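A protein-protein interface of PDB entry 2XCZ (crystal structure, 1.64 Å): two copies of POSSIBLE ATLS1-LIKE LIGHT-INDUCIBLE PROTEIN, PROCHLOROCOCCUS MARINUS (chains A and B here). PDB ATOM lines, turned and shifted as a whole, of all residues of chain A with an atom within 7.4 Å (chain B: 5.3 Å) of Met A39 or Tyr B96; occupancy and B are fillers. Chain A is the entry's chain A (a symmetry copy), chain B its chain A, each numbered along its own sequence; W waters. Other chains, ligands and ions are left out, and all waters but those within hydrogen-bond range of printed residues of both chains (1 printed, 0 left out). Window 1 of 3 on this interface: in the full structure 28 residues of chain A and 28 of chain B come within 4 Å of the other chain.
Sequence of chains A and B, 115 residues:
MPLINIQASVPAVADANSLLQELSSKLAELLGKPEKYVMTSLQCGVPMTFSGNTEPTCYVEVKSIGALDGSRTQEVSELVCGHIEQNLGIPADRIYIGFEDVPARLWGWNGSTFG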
ATOM      1  N   PRO A   2     -18.596  27.842   2.363  1.00  0.00           N
ATOM      2  CA  PRO A   2     -18.929  28.297   3.708  1.00  0.00           C
ATOM      3  C   PRO A   2     -17.878  27.931   4.742  1.00  0.00           C
ATOM      4  O   PRO A   2     -17.057  27.036   4.532  1.00  0.00           O
ATOM      5  CB  PRO A   2     -20.220  27.531   4.034  1.00  0.00           C
ATOM      6  CG  PRO A   2     -20.757  27.102   2.703  1.00  0.00           C
ATOM      7  CD  PRO A   2     -19.567  26.852   1.867  1.00  0.00           C
ATOM      8  N   LEU A   3     -17.947  28.621   5.864  1.00  0.00           N
ATOM      9  CA  LEU A   3     -17.012  28.442   6.967  1.00  0.00           C
ATOM     10  C   LEU A   3     -17.818  28.460   8.252  1.00  0.00           C
ATOM     11  O   LEU A   3     -18.688  29.313   8.438  1.00  0.00           O
ATOM     12  CB  LEU A   3     -16.004  29.599   6.982  1.00  0.00           C
ATOM     13  CG  LEU A   3     -15.042  29.678   8.166  1.00  0.00           C
ATOM     14  CD1 LEU A   3     -13.968  28.615   8.128  1.00  0.00           C
ATOM     15  CD2 LEU A   3     -14.416  31.066   8.198  1.00  0.00           C
ATOM     16  N   ILE A   4     -17.555  27.483   9.118  1.00  0.00           N
ATOM     17  CA  ILE A   4     -18.089  27.503  10.476  1.00  0.00           C
ATOM     18  C   ILE A   4     -17.002  27.147  11.503  1.00  0.00           C
ATOM     19  O   ILE A   4     -16.507  26.021  11.545  1.00  0.00           O
ATOM     20  CB  ILE A   4     -19.372  26.651  10.603  1.00  0.00           C
ATOM     21  CG1 ILE A   4     -19.945  26.721  12.030  1.00  0.00           C
ATOM     22  CG2 ILE A   4     -19.143  25.201  10.087  1.00  0.00           C
ATOM     23  CD1 ILE A   4     -21.404  26.265  12.121  1.00  0.00           C
ATOM     24  N   ASN A   5     -16.654  28.132  12.332  1.00  0.00           N
ATOM     25  CA  ASN A   5     -15.629  27.965  13.359  1.00  0.00           C
ATOM     26  C   ASN A   5     -16.298  28.010  14.732  1.00  0.00           C
ATOM     27  O   ASN A   5     -16.973  28.987  15.058  1.00  0.00           O
ATOM     28  CB  ASN A   5     -14.584  29.086  13.236  1.00  0.00           C
ATOM     29  CG  ASN A   5     -13.682  28.938  12.022  1.00  0.00           C
ATOM     30  OD1 ASN A   5     -13.255  27.832  11.656  1.00  0.00           O
ATOM     31  ND2 ASN A   5     -13.354  30.074  11.413  1.00  0.00           N
ATOM     32  N   LEU A  20     -18.087  17.357  13.476  1.00  0.00           N
ATOM     33  CA  LEU A  20     -17.815  18.348  12.428  1.00  0.00           C
ATOM     34  C   LEU A  20     -18.243  17.853  11.049  1.00  0.00           C
ATOM     35  O   LEU A  20     -18.791  18.616  10.249  1.00  0.00           O
ATOM     36  CB  LEU A  20     -16.332  18.726  12.419  1.00  0.00           C
ATOM     37  CG  LEU A  20     -15.851  19.569  13.613  1.00  0.00           C
ATOM     38  CD1 LEU A  20     -14.338  19.771  13.549  1.00  0.00           C
ATOM     39  CD2 LEU A  20     -16.569  20.927  13.713  1.00  0.00           C
ATOM     40  N   SER A  24     -20.881  19.618   8.743  1.00  0.00           N
ATOM     41  CA  SER A  24     -20.439  19.988   7.406  1.00  0.00           C
ATOM     42  C   SER A  24     -21.473  19.634   6.326  1.00  0.00           C
ATOM     43  O   SER A  24     -21.827  20.477   5.496  1.00  0.00           O
ATOM     44  CB  SER A  24     -19.093  19.319   7.101  1.00  0.00           C
ATOM     45  OG  SER A  24     -18.666  19.599   5.784  1.00  0.00           O
ATOM     46  N   LEU A  27     -24.790  21.679   6.898  1.00  0.00           N
ATOM     47  CA  LEU A  27     -24.607  23.057   6.459  1.00  0.00           C
ATOM     48  C   LEU A  27     -24.548  23.197   4.936  1.00  0.00           C
ATOM     49  O   LEU A  27     -25.113  24.137   4.372  1.00  0.00           O
ATOM     50  CB  LEU A  27     -23.405  23.727   7.154  1.00  0.00           C
ATOM     51  CG  LEU A  27     -23.287  25.245   6.922  1.00  0.00           C
ATOM     52  CD1 LEU A  27     -24.452  26.011   7.573  1.00  0.00           C
ATOM     53  CD2 LEU A  27     -21.951  25.781   7.436  1.00  0.00           C
ATOM     54  N   PRO A  34     -22.015  23.026  -2.546  1.00  0.00           N
ATOM     55  CA  PRO A  34     -21.316  21.749  -2.577  1.00  0.00           C
ATOM     56  C   PRO A  34     -20.505  21.583  -1.292  1.00  0.00           C
ATOM     57  O   PRO A  34     -19.808  22.535  -0.873  1.00  0.00           O
ATOM     58  CB  PRO A  34     -20.363  21.881  -3.781  1.00  0.00           C
ATOM     59  CG  PRO A  34     -20.874  23.013  -4.585  1.00  0.00           C
ATOM     60  CD  PRO A  34     -21.574  23.935  -3.625  1.00  0.00           C
ATOM     61  N   GLU A  35     -20.594  20.410  -0.667  1.00  0.00           N
ATOM     62  CA  GLU A  35     -19.844  20.181   0.564  1.00  0.00           C
ATOM     63  C   GLU A  35     -18.333  20.320   0.394  1.00  0.00           C
ATOM     64  O   GLU A  35     -17.638  20.626   1.363  1.00  0.00           O
ATOM     65  CB  GLU A  35     -20.183  18.851   1.222  1.00  0.00           C
ATOM     66  CG  GLU A  35     -19.754  18.847   2.689  1.00  0.00           C
ATOM     67  CD  GLU A  35     -19.943  17.524   3.376  1.00  0.00           C
ATOM     68  OE1 GLU A  35     -19.369  17.351   4.466  1.00  0.00           O
ATOM     69  OE2 GLU A  35     -20.661  16.654   2.833  1.00  0.00           O
ATOM     70  N   LYS A  36     -17.842  20.109  -0.831  1.00  0.00           N
ATOM     71  CA  LYS A  36     -16.436  20.379  -1.162  1.00  0.00           C
ATOM     72  C   LYS A  36     -15.957  21.704  -0.552  1.00  0.00           C
ATOM     73  O   LYS A  36     -14.829  21.787  -0.052  1.00  0.00           O
ATOM     74  CB  LYS A  36     -16.230  20.423  -2.679  1.00  0.00           C
ATOM     75  CG  LYS A  36     -14.787  20.641  -3.093  1.00  0.00           C
ATOM     76  CD  LYS A  36     -14.704  20.959  -4.574  1.00  0.00           C
ATOM     77  CE  LYS A  36     -13.282  21.291  -5.016  1.00  0.00           C
ATOM     78  NZ  LYS A  36     -12.369  20.127  -4.853  1.00  0.00           N
ATOM     79  N   TYR A  37     -16.820  22.715  -0.589  1.00  0.00           N
ATOM     80  CA  TYR A  37     -16.427  24.077  -0.206  1.00  0.00           C
ATOM     81  C   TYR A  37     -16.700  24.440   1.248  1.00  0.00           C
ATOM     82  O   TYR A  37     -16.439  25.564   1.661  1.00  0.00           O
ATOM     83  CB  TYR A  37     -17.060  25.102  -1.141  1.00  0.00           C
ATOM     84  CG  TYR A  37     -16.527  24.987  -2.554  1.00  0.00           C
ATOM     85  CD1 TYR A  37     -15.215  25.363  -2.858  1.00  0.00           C
ATOM     86  CD2 TYR A  37     -17.318  24.472  -3.570  1.00  0.00           C
ATOM     87  CE1 TYR A  37     -14.703  25.233  -4.160  1.00  0.00           C
ATOM     88  CE2 TYR A  37     -16.819  24.340  -4.879  1.00  0.00           C
ATOM     89  CZ  TYR A  37     -15.514  24.722  -5.164  1.00  0.00           C
ATOM     90  OH  TYR A  37     -15.027  24.592  -6.454  1.00  0.00           O
ATOM     91  N   VAL A  38     -17.187  23.487   2.026  1.00  0.00           N
ATOM     92  CA  VAL A  38     -17.464  23.766   3.442  1.00  0.00           C
ATOM     93  C   VAL A  38     -16.245  23.488   4.312  1.00  0.00           C
ATOM     94  O   VAL A  38     -15.680  22.385   4.290  1.00  0.00           O
ATOM     95  CB  VAL A  38     -18.666  22.927   3.980  1.00  0.00           C
ATOM     96  CG1 VAL A  38     -18.880  23.163   5.480  1.00  0.00           C
ATOM     97  CG2 VAL A  38     -19.928  23.240   3.212  1.00  0.00           C
ATOM     98  N   MET A  39     -15.871  24.491   5.111  1.00  0.00           N
ATOM     99  CA  MET A  39     -14.780  24.355   6.077  1.00  0.00           C
ATOM    100  C   MET A  39     -15.330  24.493   7.480  1.00  0.00           C
ATOM    101  O   MET A  39     -16.138  25.384   7.750  1.00  0.00           O
ATOM    102  CB  MET A  39     -13.718  25.428   5.831  1.00  0.00           C
ATOM    103  CG  MET A  39     -12.484  25.312   6.737  1.00  0.00           C
ATOM    104  SD  MET A  39     -11.150  26.445   6.297  1.00  0.00           S
ATOM    105  CE  MET A  39     -10.513  25.646   4.829  1.00  0.00           C
ATOM    106  N   THR A  40     -14.879  23.630   8.388  1.00  0.00           N
ATOM    107  CA  THR A  40     -15.371  23.662   9.771  1.00  0.00           C
ATOM    108  C   THR A  40     -14.213  23.566  10.759  1.00  0.00           C
ATOM    109  O   THR A  40     -13.139  23.066  10.423  1.00  0.00           O
ATOM    110  CB  THR A  40     -16.382  22.504  10.103  1.00  0.00           C
ATOM    111  OG1 THR A  40     -15.666  21.282  10.330  1.00  0.00           O
ATOM    112  CG2 THR A  40     -17.417  22.287   8.985  1.00  0.00           C
ATOM    113  N   SER A  41     -14.440  24.051  11.969  1.00  0.00           N
ATOM    114  CA  SER A  41     -13.495  23.816  13.067  1.00  0.00           C
ATOM    115  C   SER A  41     -14.178  23.781  14.424  1.00  0.00           C
ATOM    116  O   SER A  41     -15.265  24.343  14.610  1.00  0.00           O
ATOM    117  CB  SER A  41     -12.387  24.876  13.075  1.00  0.00           C
ATOM    118  OG  SER A  41     -12.870  26.141  13.454  1.00  0.00           O
ATOM    119  N   GLU A  61     -18.479  31.354  14.602  1.00  0.00           N
ATOM    120  CA  GLU A  61     -18.537  32.245  13.437  1.00  0.00           C
ATOM    121  C   GLU A  61     -18.906  31.481  12.178  1.00  0.00           C
ATOM    122  O   GLU A  61     -18.391  30.390  11.926  1.00  0.00           O
ATOM    123  CB  GLU A  61     -17.285  33.074  13.258  1.00  0.00           C
ATOM    124  CG  GLU A  61     -16.014  32.357  13.323  1.00  0.00           C
ATOM    125  CD  GLU A  61     -14.843  33.223  12.842  1.00  0.00           C
ATOM    126  OE1 GLU A  61     -14.814  34.454  13.129  1.00  0.00           O
ATOM    127  OE2 GLU A  61     -13.954  32.658  12.191  1.00  0.00           O
ATOM    128  N   LYS A  63     -19.413  32.069   8.002  1.00  0.00           N
ATOM    129  CA  LYS A  63     -19.244  32.923   6.823  1.00  0.00           C
ATOM    130  C   LYS A  63     -19.671  32.177   5.571  1.00  0.00           C
ATOM    131  O   LYS A  63     -19.551  30.960   5.472  1.00  0.00           O
ATOM    132  CB  LYS A  63     -17.798  33.421   6.672  1.00  0.00           C
ATOM    133  CG  LYS A  63     -17.275  34.217   7.857  1.00  0.00           C
ATOM    134  CD  LYS A  63     -15.871  34.728   7.569  1.00  0.00           C
ATOM    135  CE  LYS A  63     -15.258  35.424   8.779  1.00  0.00           C
ATOM    136  NZ  LYS A  63     -16.140  36.483   9.376  1.00  0.00           N
ATOM    137  N   ILE A  65     -20.136  33.040   1.024  1.00  0.00           N
ATOM    138  CA  ILE A  65     -20.303  33.925  -0.112  1.00  0.00           C
ATOM    139  C   ILE A  65     -21.775  33.806  -0.500  1.00  0.00           C
ATOM    140  O   ILE A  65     -22.200  32.823  -1.116  1.00  0.00           O
ATOM    141  CB  ILE A  65     -19.359  33.574  -1.295  1.00  0.00           C
ATOM    142  CG1 ILE A  65     -17.889  33.753  -0.902  1.00  0.00           C
ATOM    143  CG2 ILE A  65     -19.681  34.468  -2.504  1.00  0.00           C
ATOM    144  CD1 ILE A  65     -16.913  33.163  -1.916  1.00  0.00           C
ATOM    145  N   TRP A 107     -12.523  36.488  -0.318  1.00  0.00           N
ATOM    146  CA  TRP A 107     -12.445  35.110   0.115  1.00  0.00           C
ATOM    147  C   TRP A 107     -11.330  34.413  -0.663  1.00  0.00           C
ATOM    148  O   TRP A 107     -11.492  34.076  -1.840  1.00  0.00           O
ATOM    149  CB  TRP A 107     -13.791  34.393  -0.094  1.00  0.00           C
ATOM    150  CG  TRP A 107     -13.901  33.089   0.680  1.00  0.00           C
ATOM    151  CD1 TRP A 107     -13.031  32.027   0.647  1.00  0.00           C
ATOM    152  CD2 TRP A 107     -14.914  32.745   1.626  1.00  0.00           C
ATOM    153  NE1 TRP A 107     -13.452  31.043   1.513  1.00  0.00           N
ATOM    154  CE2 TRP A 107     -14.606  31.457   2.124  1.00  0.00           C
ATOM    155  CE3 TRP A 107     -16.046  33.406   2.113  1.00  0.00           C
ATOM    156  CZ2 TRP A 107     -15.405  30.802   3.068  1.00  0.00           C
ATOM    157  CZ3 TRP A 107     -16.850  32.759   3.051  1.00  0.00           C
ATOM    158  CH2 TRP A 107     -16.514  31.466   3.527  1.00  0.00           C
ATOM    159  N   GLY A 108     -10.212  34.179   0.013  1.00  0.00           N
ATOM    160  CA  GLY A 108      -9.071  33.522  -0.615  1.00  0.00           C
ATOM    161  C   GLY A 108      -9.154  32.018  -0.568  1.00  0.00           C
ATOM    162  O   GLY A 108      -9.653  31.439   0.396  1.00  0.00           O
ATOM    163  N   TRP A 109      -8.686  31.374  -1.635  1.00  0.00           N
ATOM    164  CA  TRP A 109      -8.662  29.921  -1.699  1.00  0.00           C
ATOM    165  C   TRP A 109      -7.696  29.542  -2.816  1.00  0.00           C
ATOM    166  O   TRP A 109      -7.689  30.181  -3.865  1.00  0.00           O
ATOM    167  CB  TRP A 109     -10.062  29.364  -1.982  1.00  0.00           C
ATOM    168  CG  TRP A 109     -10.049  27.899  -2.270  1.00  0.00           C
ATOM    169  CD1 TRP A 109      -9.642  26.918  -1.427  1.00  0.00           C
ATOM    170  CD2 TRP A 109     -10.433  27.255  -3.489  1.00  0.00           C
ATOM    171  NE1 TRP A 109      -9.756  25.692  -2.033  1.00  0.00           N
ATOM    172  CE2 TRP A 109     -10.244  25.869  -3.302  1.00  0.00           C
ATOM    173  CE3 TRP A 109     -10.921  27.714  -4.720  1.00  0.00           C
ATOM    174  CZ2 TRP A 109     -10.526  24.922  -4.307  1.00  0.00           C
ATOM    175  CZ3 TRP A 109     -11.209  26.773  -5.721  1.00  0.00           C
ATOM    176  CH2 TRP A 109     -11.001  25.393  -5.505  1.00  0.00           C
ATOM    177  N   ASN A 110      -6.845  28.546  -2.562  1.00  0.00           N
ATOM    178  CA  ASN A 110      -5.992  27.982  -3.621  1.00  0.00           C
ATOM    179  C   ASN A 110      -5.099  29.016  -4.344  1.00  0.00           C
ATOM    180  O   ASN A 110      -4.991  29.024  -5.582  1.00  0.00           O
ATOM    181  CB  ASN A 110      -6.867  27.208  -4.621  1.00  0.00           C
ATOM    182  CG  ASN A 110      -6.062  26.265  -5.509  1.00  0.00           C
ATOM    183  OD1 ASN A 110      -4.986  25.785  -5.128  1.00  0.00           O
ATOM    184  ND2 ASN A 110      -6.593  25.984  -6.698  1.00  0.00           N
ATOM    185  N   PHE A 114     -12.174  33.872  -4.818  1.00  0.00           N
ATOM    186  CA  PHE A 114     -13.364  33.433  -5.556  1.00  0.00           C
ATOM    187  C   PHE A 114     -13.925  34.518  -6.486  1.00  0.00           C
ATOM    188  O   PHE A 114     -14.885  34.270  -7.226  1.00  0.00           O
ATOM    189  CB  PHE A 114     -14.460  32.954  -4.588  1.00  0.00           C
ATOM    190  CG  PHE A 114     -14.256  31.554  -4.071  1.00  0.00           C
ATOM    191  CD1 PHE A 114     -13.747  31.331  -2.798  1.00  0.00           C
ATOM    192  CD2 PHE A 114     -14.607  30.447  -4.857  1.00  0.00           C
ATOM    193  CE1 PHE A 114     -13.576  30.039  -2.316  1.00  0.00           C
ATOM    194  CE2 PHE A 114     -14.430  29.149  -4.389  1.00  0.00           C
ATOM    195  CZ  PHE A 114     -13.912  28.940  -3.116  1.00  0.00           C
ATOM    196  N   MET B  48     -10.429  20.230  12.496  1.00  0.00           N
ATOM    197  CA  MET B  48     -11.049  20.890  11.343  1.00  0.00           C
ATOM    198  C   MET B  48     -11.459  19.862  10.309  1.00  0.00           C
ATOM    199  O   MET B  48     -10.843  18.793  10.206  1.00  0.00           O
ATOM    200  CB  MET B  48     -10.056  21.845  10.683  1.00  0.00           C
ATOM    201  CG  MET B  48      -9.698  23.034  11.540  1.00  0.00           C
ATOM    202  SD  MET B  48      -8.676  24.208  10.663  1.00  0.00           S
ATOM    203  CE  MET B  48      -9.821  24.815   9.415  1.00  0.00           C
ATOM    204  N   THR B  49     -12.502  20.176   9.554  1.00  0.00           N
ATOM    205  CA  THR B  49     -12.767  19.466   8.306  1.00  0.00           C
ATOM    206  C   THR B  49     -12.769  20.446   7.133  1.00  0.00           C
ATOM    207  O   THR B  49     -13.023  21.637   7.302  1.00  0.00           O
ATOM    208  CB  THR B  49     -14.096  18.669   8.321  1.00  0.00           C
ATOM    209  OG1 THR B  49     -15.211  19.568   8.301  1.00  0.00           O
ATOM    210  CG2 THR B  49     -14.178  17.775   9.546  1.00  0.00           C
ATOM    211  N   PHE B  50     -12.462  19.936   5.946  1.00  0.00           N
ATOM    212  CA  PHE B  50     -12.698  20.671   4.711  1.00  0.00           C
ATOM    213  C   PHE B  50     -13.112  19.640   3.665  1.00  0.00           C
ATOM    214  O   PHE B  50     -12.507  18.562   3.588  1.00  0.00           O
ATOM    215  CB  PHE B  50     -11.459  21.454   4.259  1.00  0.00           C
ATOM    216  CG  PHE B  50     -11.701  22.305   3.047  1.00  0.00           C
ATOM    217  CD1 PHE B  50     -12.748  23.231   3.024  1.00  0.00           C
ATOM    218  CD2 PHE B  50     -10.907  22.161   1.913  1.00  0.00           C
ATOM    219  CE1 PHE B  50     -12.986  24.018   1.906  1.00  0.00           C
ATOM    220  CE2 PHE B  50     -11.137  22.942   0.782  1.00  0.00           C
ATOM    221  CZ  PHE B  50     -12.179  23.877   0.778  1.00  0.00           C
ATOM    222  N   THR B  57      -5.646  21.072   6.677  1.00  0.00           N
ATOM    223  CA  THR B  57      -6.435  22.215   6.212  1.00  0.00           C
ATOM    224  C   THR B  57      -6.195  23.429   7.110  1.00  0.00           C
ATOM    225  O   THR B  57      -5.677  23.301   8.228  1.00  0.00           O
ATOM    226  CB  THR B  57      -7.923  21.874   6.105  1.00  0.00           C
ATOM    227  OG1 THR B  57      -8.613  22.977   5.503  1.00  0.00           O
ATOM    228  CG2 THR B  57      -8.524  21.574   7.463  1.00  0.00           C
ATOM    229  N   CYS B  58      -6.582  24.609   6.623  1.00  0.00           N
ATOM    230  CA  CYS B  58      -6.143  25.840   7.239  1.00  0.00           C
ATOM    231  C   CYS B  58      -7.179  26.941   7.002  1.00  0.00           C
ATOM    232  O   CYS B  58      -7.651  27.088   5.883  1.00  0.00           O
ATOM    233  CB  CYS B  58      -4.824  26.211   6.549  1.00  0.00           C
ATOM    234  SG  CYS B  58      -4.074  27.630   7.074  1.00  0.00           S
ATOM    235  N   TYR B  59      -7.549  27.683   8.052  1.00  0.00           N
ATOM    236  CA  TYR B  59      -8.298  28.933   7.868  1.00  0.00           C
ATOM    237  C   TYR B  59      -7.459  30.128   8.293  1.00  0.00           C
ATOM    238  O   TYR B  59      -6.928  30.153   9.399  1.00  0.00           O
ATOM    239  CB  TYR B  59      -9.617  28.958   8.654  1.00  0.00           C
ATOM    240  CG  TYR B  59     -10.313  30.305   8.520  1.00  0.00           C
ATOM    241  CD1 TYR B  59     -10.779  30.741   7.281  1.00  0.00           C
ATOM    242  CD2 TYR B  59     -10.446  31.157   9.625  1.00  0.00           C
ATOM    243  CE1 TYR B  59     -11.380  31.986   7.140  1.00  0.00           C
ATOM    244  CE2 TYR B  59     -11.053  32.424   9.500  1.00  0.00           C
ATOM    245  CZ  TYR B  59     -11.503  32.821   8.248  1.00  0.00           C
ATOM    246  OH  TYR B  59     -12.112  34.054   8.112  1.00  0.00           O
ATOM    247  N   VAL B  60      -7.397  31.146   7.443  1.00  0.00           N
ATOM    248  CA  VAL B  60      -6.633  32.349   7.771  1.00  0.00           C
ATOM    249  C   VAL B  60      -7.553  33.558   7.781  1.00  0.00           C
ATOM    250  O   VAL B  60      -8.365  33.710   6.881  1.00  0.00           O
ATOM    251  CB  VAL B  60      -5.543  32.605   6.711  1.00  0.00           C
ATOM    252  CG1 VAL B  60      -4.642  33.798   7.119  1.00  0.00           C
ATOM    253  CG2 VAL B  60      -4.700  31.332   6.484  1.00  0.00           C
ATOM    254  N   ARG B  94      -6.565  23.502   0.114  1.00  0.00           N
ATOM    255  CA  ARG B  94      -7.248  23.286   1.390  1.00  0.00           C
ATOM    256  C   ARG B  94      -7.081  24.481   2.340  1.00  0.00           C
ATOM    257  O   ARG B  94      -7.218  24.352   3.565  1.00  0.00           O
ATOM    258  CB  ARG B  94      -6.801  21.965   2.019  1.00  0.00           C
ATOM    259  CG  ARG B  94      -7.379  20.764   1.234  1.00  0.00           C
ATOM    260  CD  ARG B  94      -7.043  19.423   1.868  1.00  0.00           C
ATOM    261  NE  ARG B  94      -7.681  19.188   3.166  1.00  0.00           N
ATOM    262  CZ  ARG B  94      -8.954  18.837   3.351  1.00  0.00           C
ATOM    263  NH1 ARG B  94      -9.395  18.633   4.589  1.00  0.00           N
ATOM    264  NH2 ARG B  94      -9.788  18.692   2.320  1.00  0.00           N
ATOM    265  N   ILE B  95      -6.790  25.644   1.753  1.00  0.00           N
ATOM    266  CA  ILE B  95      -6.627  26.886   2.530  1.00  0.00           C
ATOM    267  C   ILE B  95      -7.710  27.898   2.175  1.00  0.00           C
ATOM    268  O   ILE B  95      -7.937  28.178   0.994  1.00  0.00           O
ATOM    269  CB  ILE B  95      -5.226  27.518   2.304  1.00  0.00           C
ATOM    270  CG1 ILE B  95      -4.122  26.508   2.680  1.00  0.00           C
ATOM    271  CG2 ILE B  95      -5.112  28.847   3.080  1.00  0.00           C
ATOM    272  CD1 ILE B  95      -2.723  26.975   2.368  1.00  0.00           C
ATOM    273  N   TYR B  96      -8.395  28.413   3.200  1.00  0.00           N
ATOM    274  CA  TYR B  96      -9.332  29.526   3.034  1.00  0.00           C
ATOM    275  C   TYR B  96      -8.782  30.753   3.744  1.00  0.00           C
ATOM    276  O   TYR B  96      -8.173  30.641   4.812  1.00  0.00           O
ATOM    277  CB  TYR B  96     -10.679  29.189   3.668  1.00  0.00           C
ATOM    278  CG  TYR B  96     -11.692  28.512   2.775  1.00  0.00           C
ATOM    279  CD1 TYR B  96     -11.469  28.353   1.412  1.00  0.00           C
ATOM    280  CD2 TYR B  96     -12.917  28.102   3.291  1.00  0.00           C
ATOM    281  CE1 TYR B  96     -12.431  27.762   0.584  1.00  0.00           C
ATOM    282  CE2 TYR B  96     -13.874  27.501   2.480  1.00  0.00           C
ATOM    283  CZ  TYR B  96     -13.629  27.346   1.132  1.00  0.00           C
ATOM    284  OH  TYR B  96     -14.580  26.773   0.305  1.00  0.00           O
ATOM    285  N   ILE B  97      -9.019  31.918   3.146  1.00  0.00           N
ATOM    286  CA  ILE B  97      -8.645  33.188   3.747  1.00  0.00           C
ATOM    287  C   ILE B  97      -9.837  34.119   3.772  1.00  0.00           C
ATOM    288  O   ILE B  97     -10.422  34.425   2.707  1.00  0.00           O
ATOM    289  CB  ILE B  97      -7.462  33.879   3.007  1.00  0.00           C
ATOM    290  CG1 ILE B  97      -6.255  32.929   2.874  1.00  0.00           C
ATOM    291  CG2 ILE B  97      -7.057  35.152   3.741  1.00  0.00           C
ATOM    292  CD1 ILE B  97      -5.207  33.443   1.889  1.00  0.00           C
ATOM    293  N   GLY B  98     -10.189  34.603   4.966  1.00  0.00           N
ATOM    294  CA  GLY B  98     -11.222  35.656   5.075  1.00  0.00           C
ATOM    295  C   GLY B  98     -10.558  37.014   5.204  1.00  0.00           C
ATOM    296  O   GLY B  98      -9.802  37.253   6.164  1.00  0.00           O
HETATM  297  O   HOH W   1     -16.091  20.115   5.708  1.00  0.00           O
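Water W1 lies within hydrogen-bond range of OG of Ser A24 (2.6 Å), O of Val A38 (2.7 Å) and OG1 of Thr B49 (2.8 Å).
Of the 12 printed residues of chain B, 10 touch a printed residue of chain A.
Of the 23 printed residues of chain A, 17 touch a printed residue of chain B.
Hydrophobic or aromatic side chains of chain A that line the printed part of chain B: Leu A3, Leu A20, Tyr A37, Met A39, Trp A107, Trp A109 and Phe A114.
Among the printed residues, 30 pairs touch across the chains.
Among the printed residues, no Asp or Glu carboxylate lies within 4 Å of a Lys or Arg side-chain nitrogen of the other chain.
No position is printed for both chains.
Of the 30 pairs that touch across the chains among the printed residues, none has its exchanged pair printed and touching as well.
O of Phe B50 lies within hydrogen-bond range of NH2 of Arg B94 (3.0 Å).
The side-chain hydroxyl (OG1) of Thr B57 sits at hydrogen-bond distance from the backbone carbonyl oxygen (O) of Arg B94, 2.8 Å away.
The backbone NH (N) of Cys B58 lies within hydrogen-bond range of the backbone carbonyl oxygen (O) of Arg B94.
N of Met A39 is in hydrogen-bond range of O of Pro A2, at 2.9 Å.
N of Ile A4 lies within hydrogen-bond range of O of Met A39 (2.9 Å).
O of Ile A4 lies within hydrogen-bond range of N of Ser A41, 2.9 Å away.
Ile A4 touches none of the printed residues of chain B.
Leu A27 touches none of the printed residues of chain B.
Printed residues of chain B within 4 Å of Lys A36: Phe B50 (3.5 Å).
Met A39 touches eight residues of chain B.
Printed residues of chain B within 4 Å of Glu A61: Tyr B59 (3.96 Å).
Printed residues of chain A within 4 Å of Cys B58: Met A39.
Printed residues of chain A within 4 Å of Arg B94: Met A39.
Printed residues of chain A within 4 Å of Tyr B96: Pro A2 (3.8 Å), Tyr A37 (2.6 Å), Met A39 (3.7 Å), Trp A107 (3.3 Å), Gly A108 (3.3 Å), Trp A109 (3.5 Å) and Phe A114 (3.9 Å).
The nearest residue of chain A that does not touch Tyr B96 is Val A38 (4.5 Å).
Among the printed residues, merely in contact across the chains: Pro A2 with Tyr B96 (3.8 Å), Leu A3 with Tyr B59 (3.3 Å), Asn A5 with Tyr B59 (3.6 Å), Leu A20 with Thr B49 (3.7 Å), Lys A36 with Phe B50 (3.5 Å), Tyr A37 with Phe B50 (3.8 Å), Val A38 with Phe B50 (3.3 Å), Met A39 with Met B48 (3.8 Å), Met A39 with Thr B49 (3.5 Å), Met A39 with Phe B50 (3.7 Å), Met A39 with Thr B57 (3.3 Å), Met A39 with Tyr B59 (3.8 Å), Met A39 with Arg B94 (3.8 Å), Met A39 with Tyr B96 (3.7 Å), Thr A40 with Met B48 (3.2 Å), Ser A41 with Met B48 (3.6 Å), Glu A61 with Tyr B59 (3.96 Å), Lys A63 with Tyr B59 (3.5 Å), Trp A107 with Tyr B96 (3.3 Å), Trp A107 with Ile B97 (3.4 Å), Gly A108 with Ile B95 (3.7 Å), Gly A108 with Tyr B96 (3.3 Å), Trp A109 with Ile B95 (3.2 Å), Trp A109 with Tyr B96 (3.5 Å), Asn A110 with Ile B95 (3.7 Å) and Phe A114 with Tyr B96 (3.9 Å).
OG1 of Thr B49 lies within hydrogen-bond range of OG1 of Thr A40 (2.7 Å).
The side-chain hydroxyl (OH) of Tyr B96 is in hydrogen-bond range of the backbone carbonyl oxygen (O) of Tyr A37 (2.6 Å).
The backbone carbonyl oxygen (O) of Ile B97 sits at hydrogen-bond distance from the backbone NH (N) of Gly A108 (2.7 Å).
O of Cys B58 lies close to SD of Met A39, 3.6 Å away.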
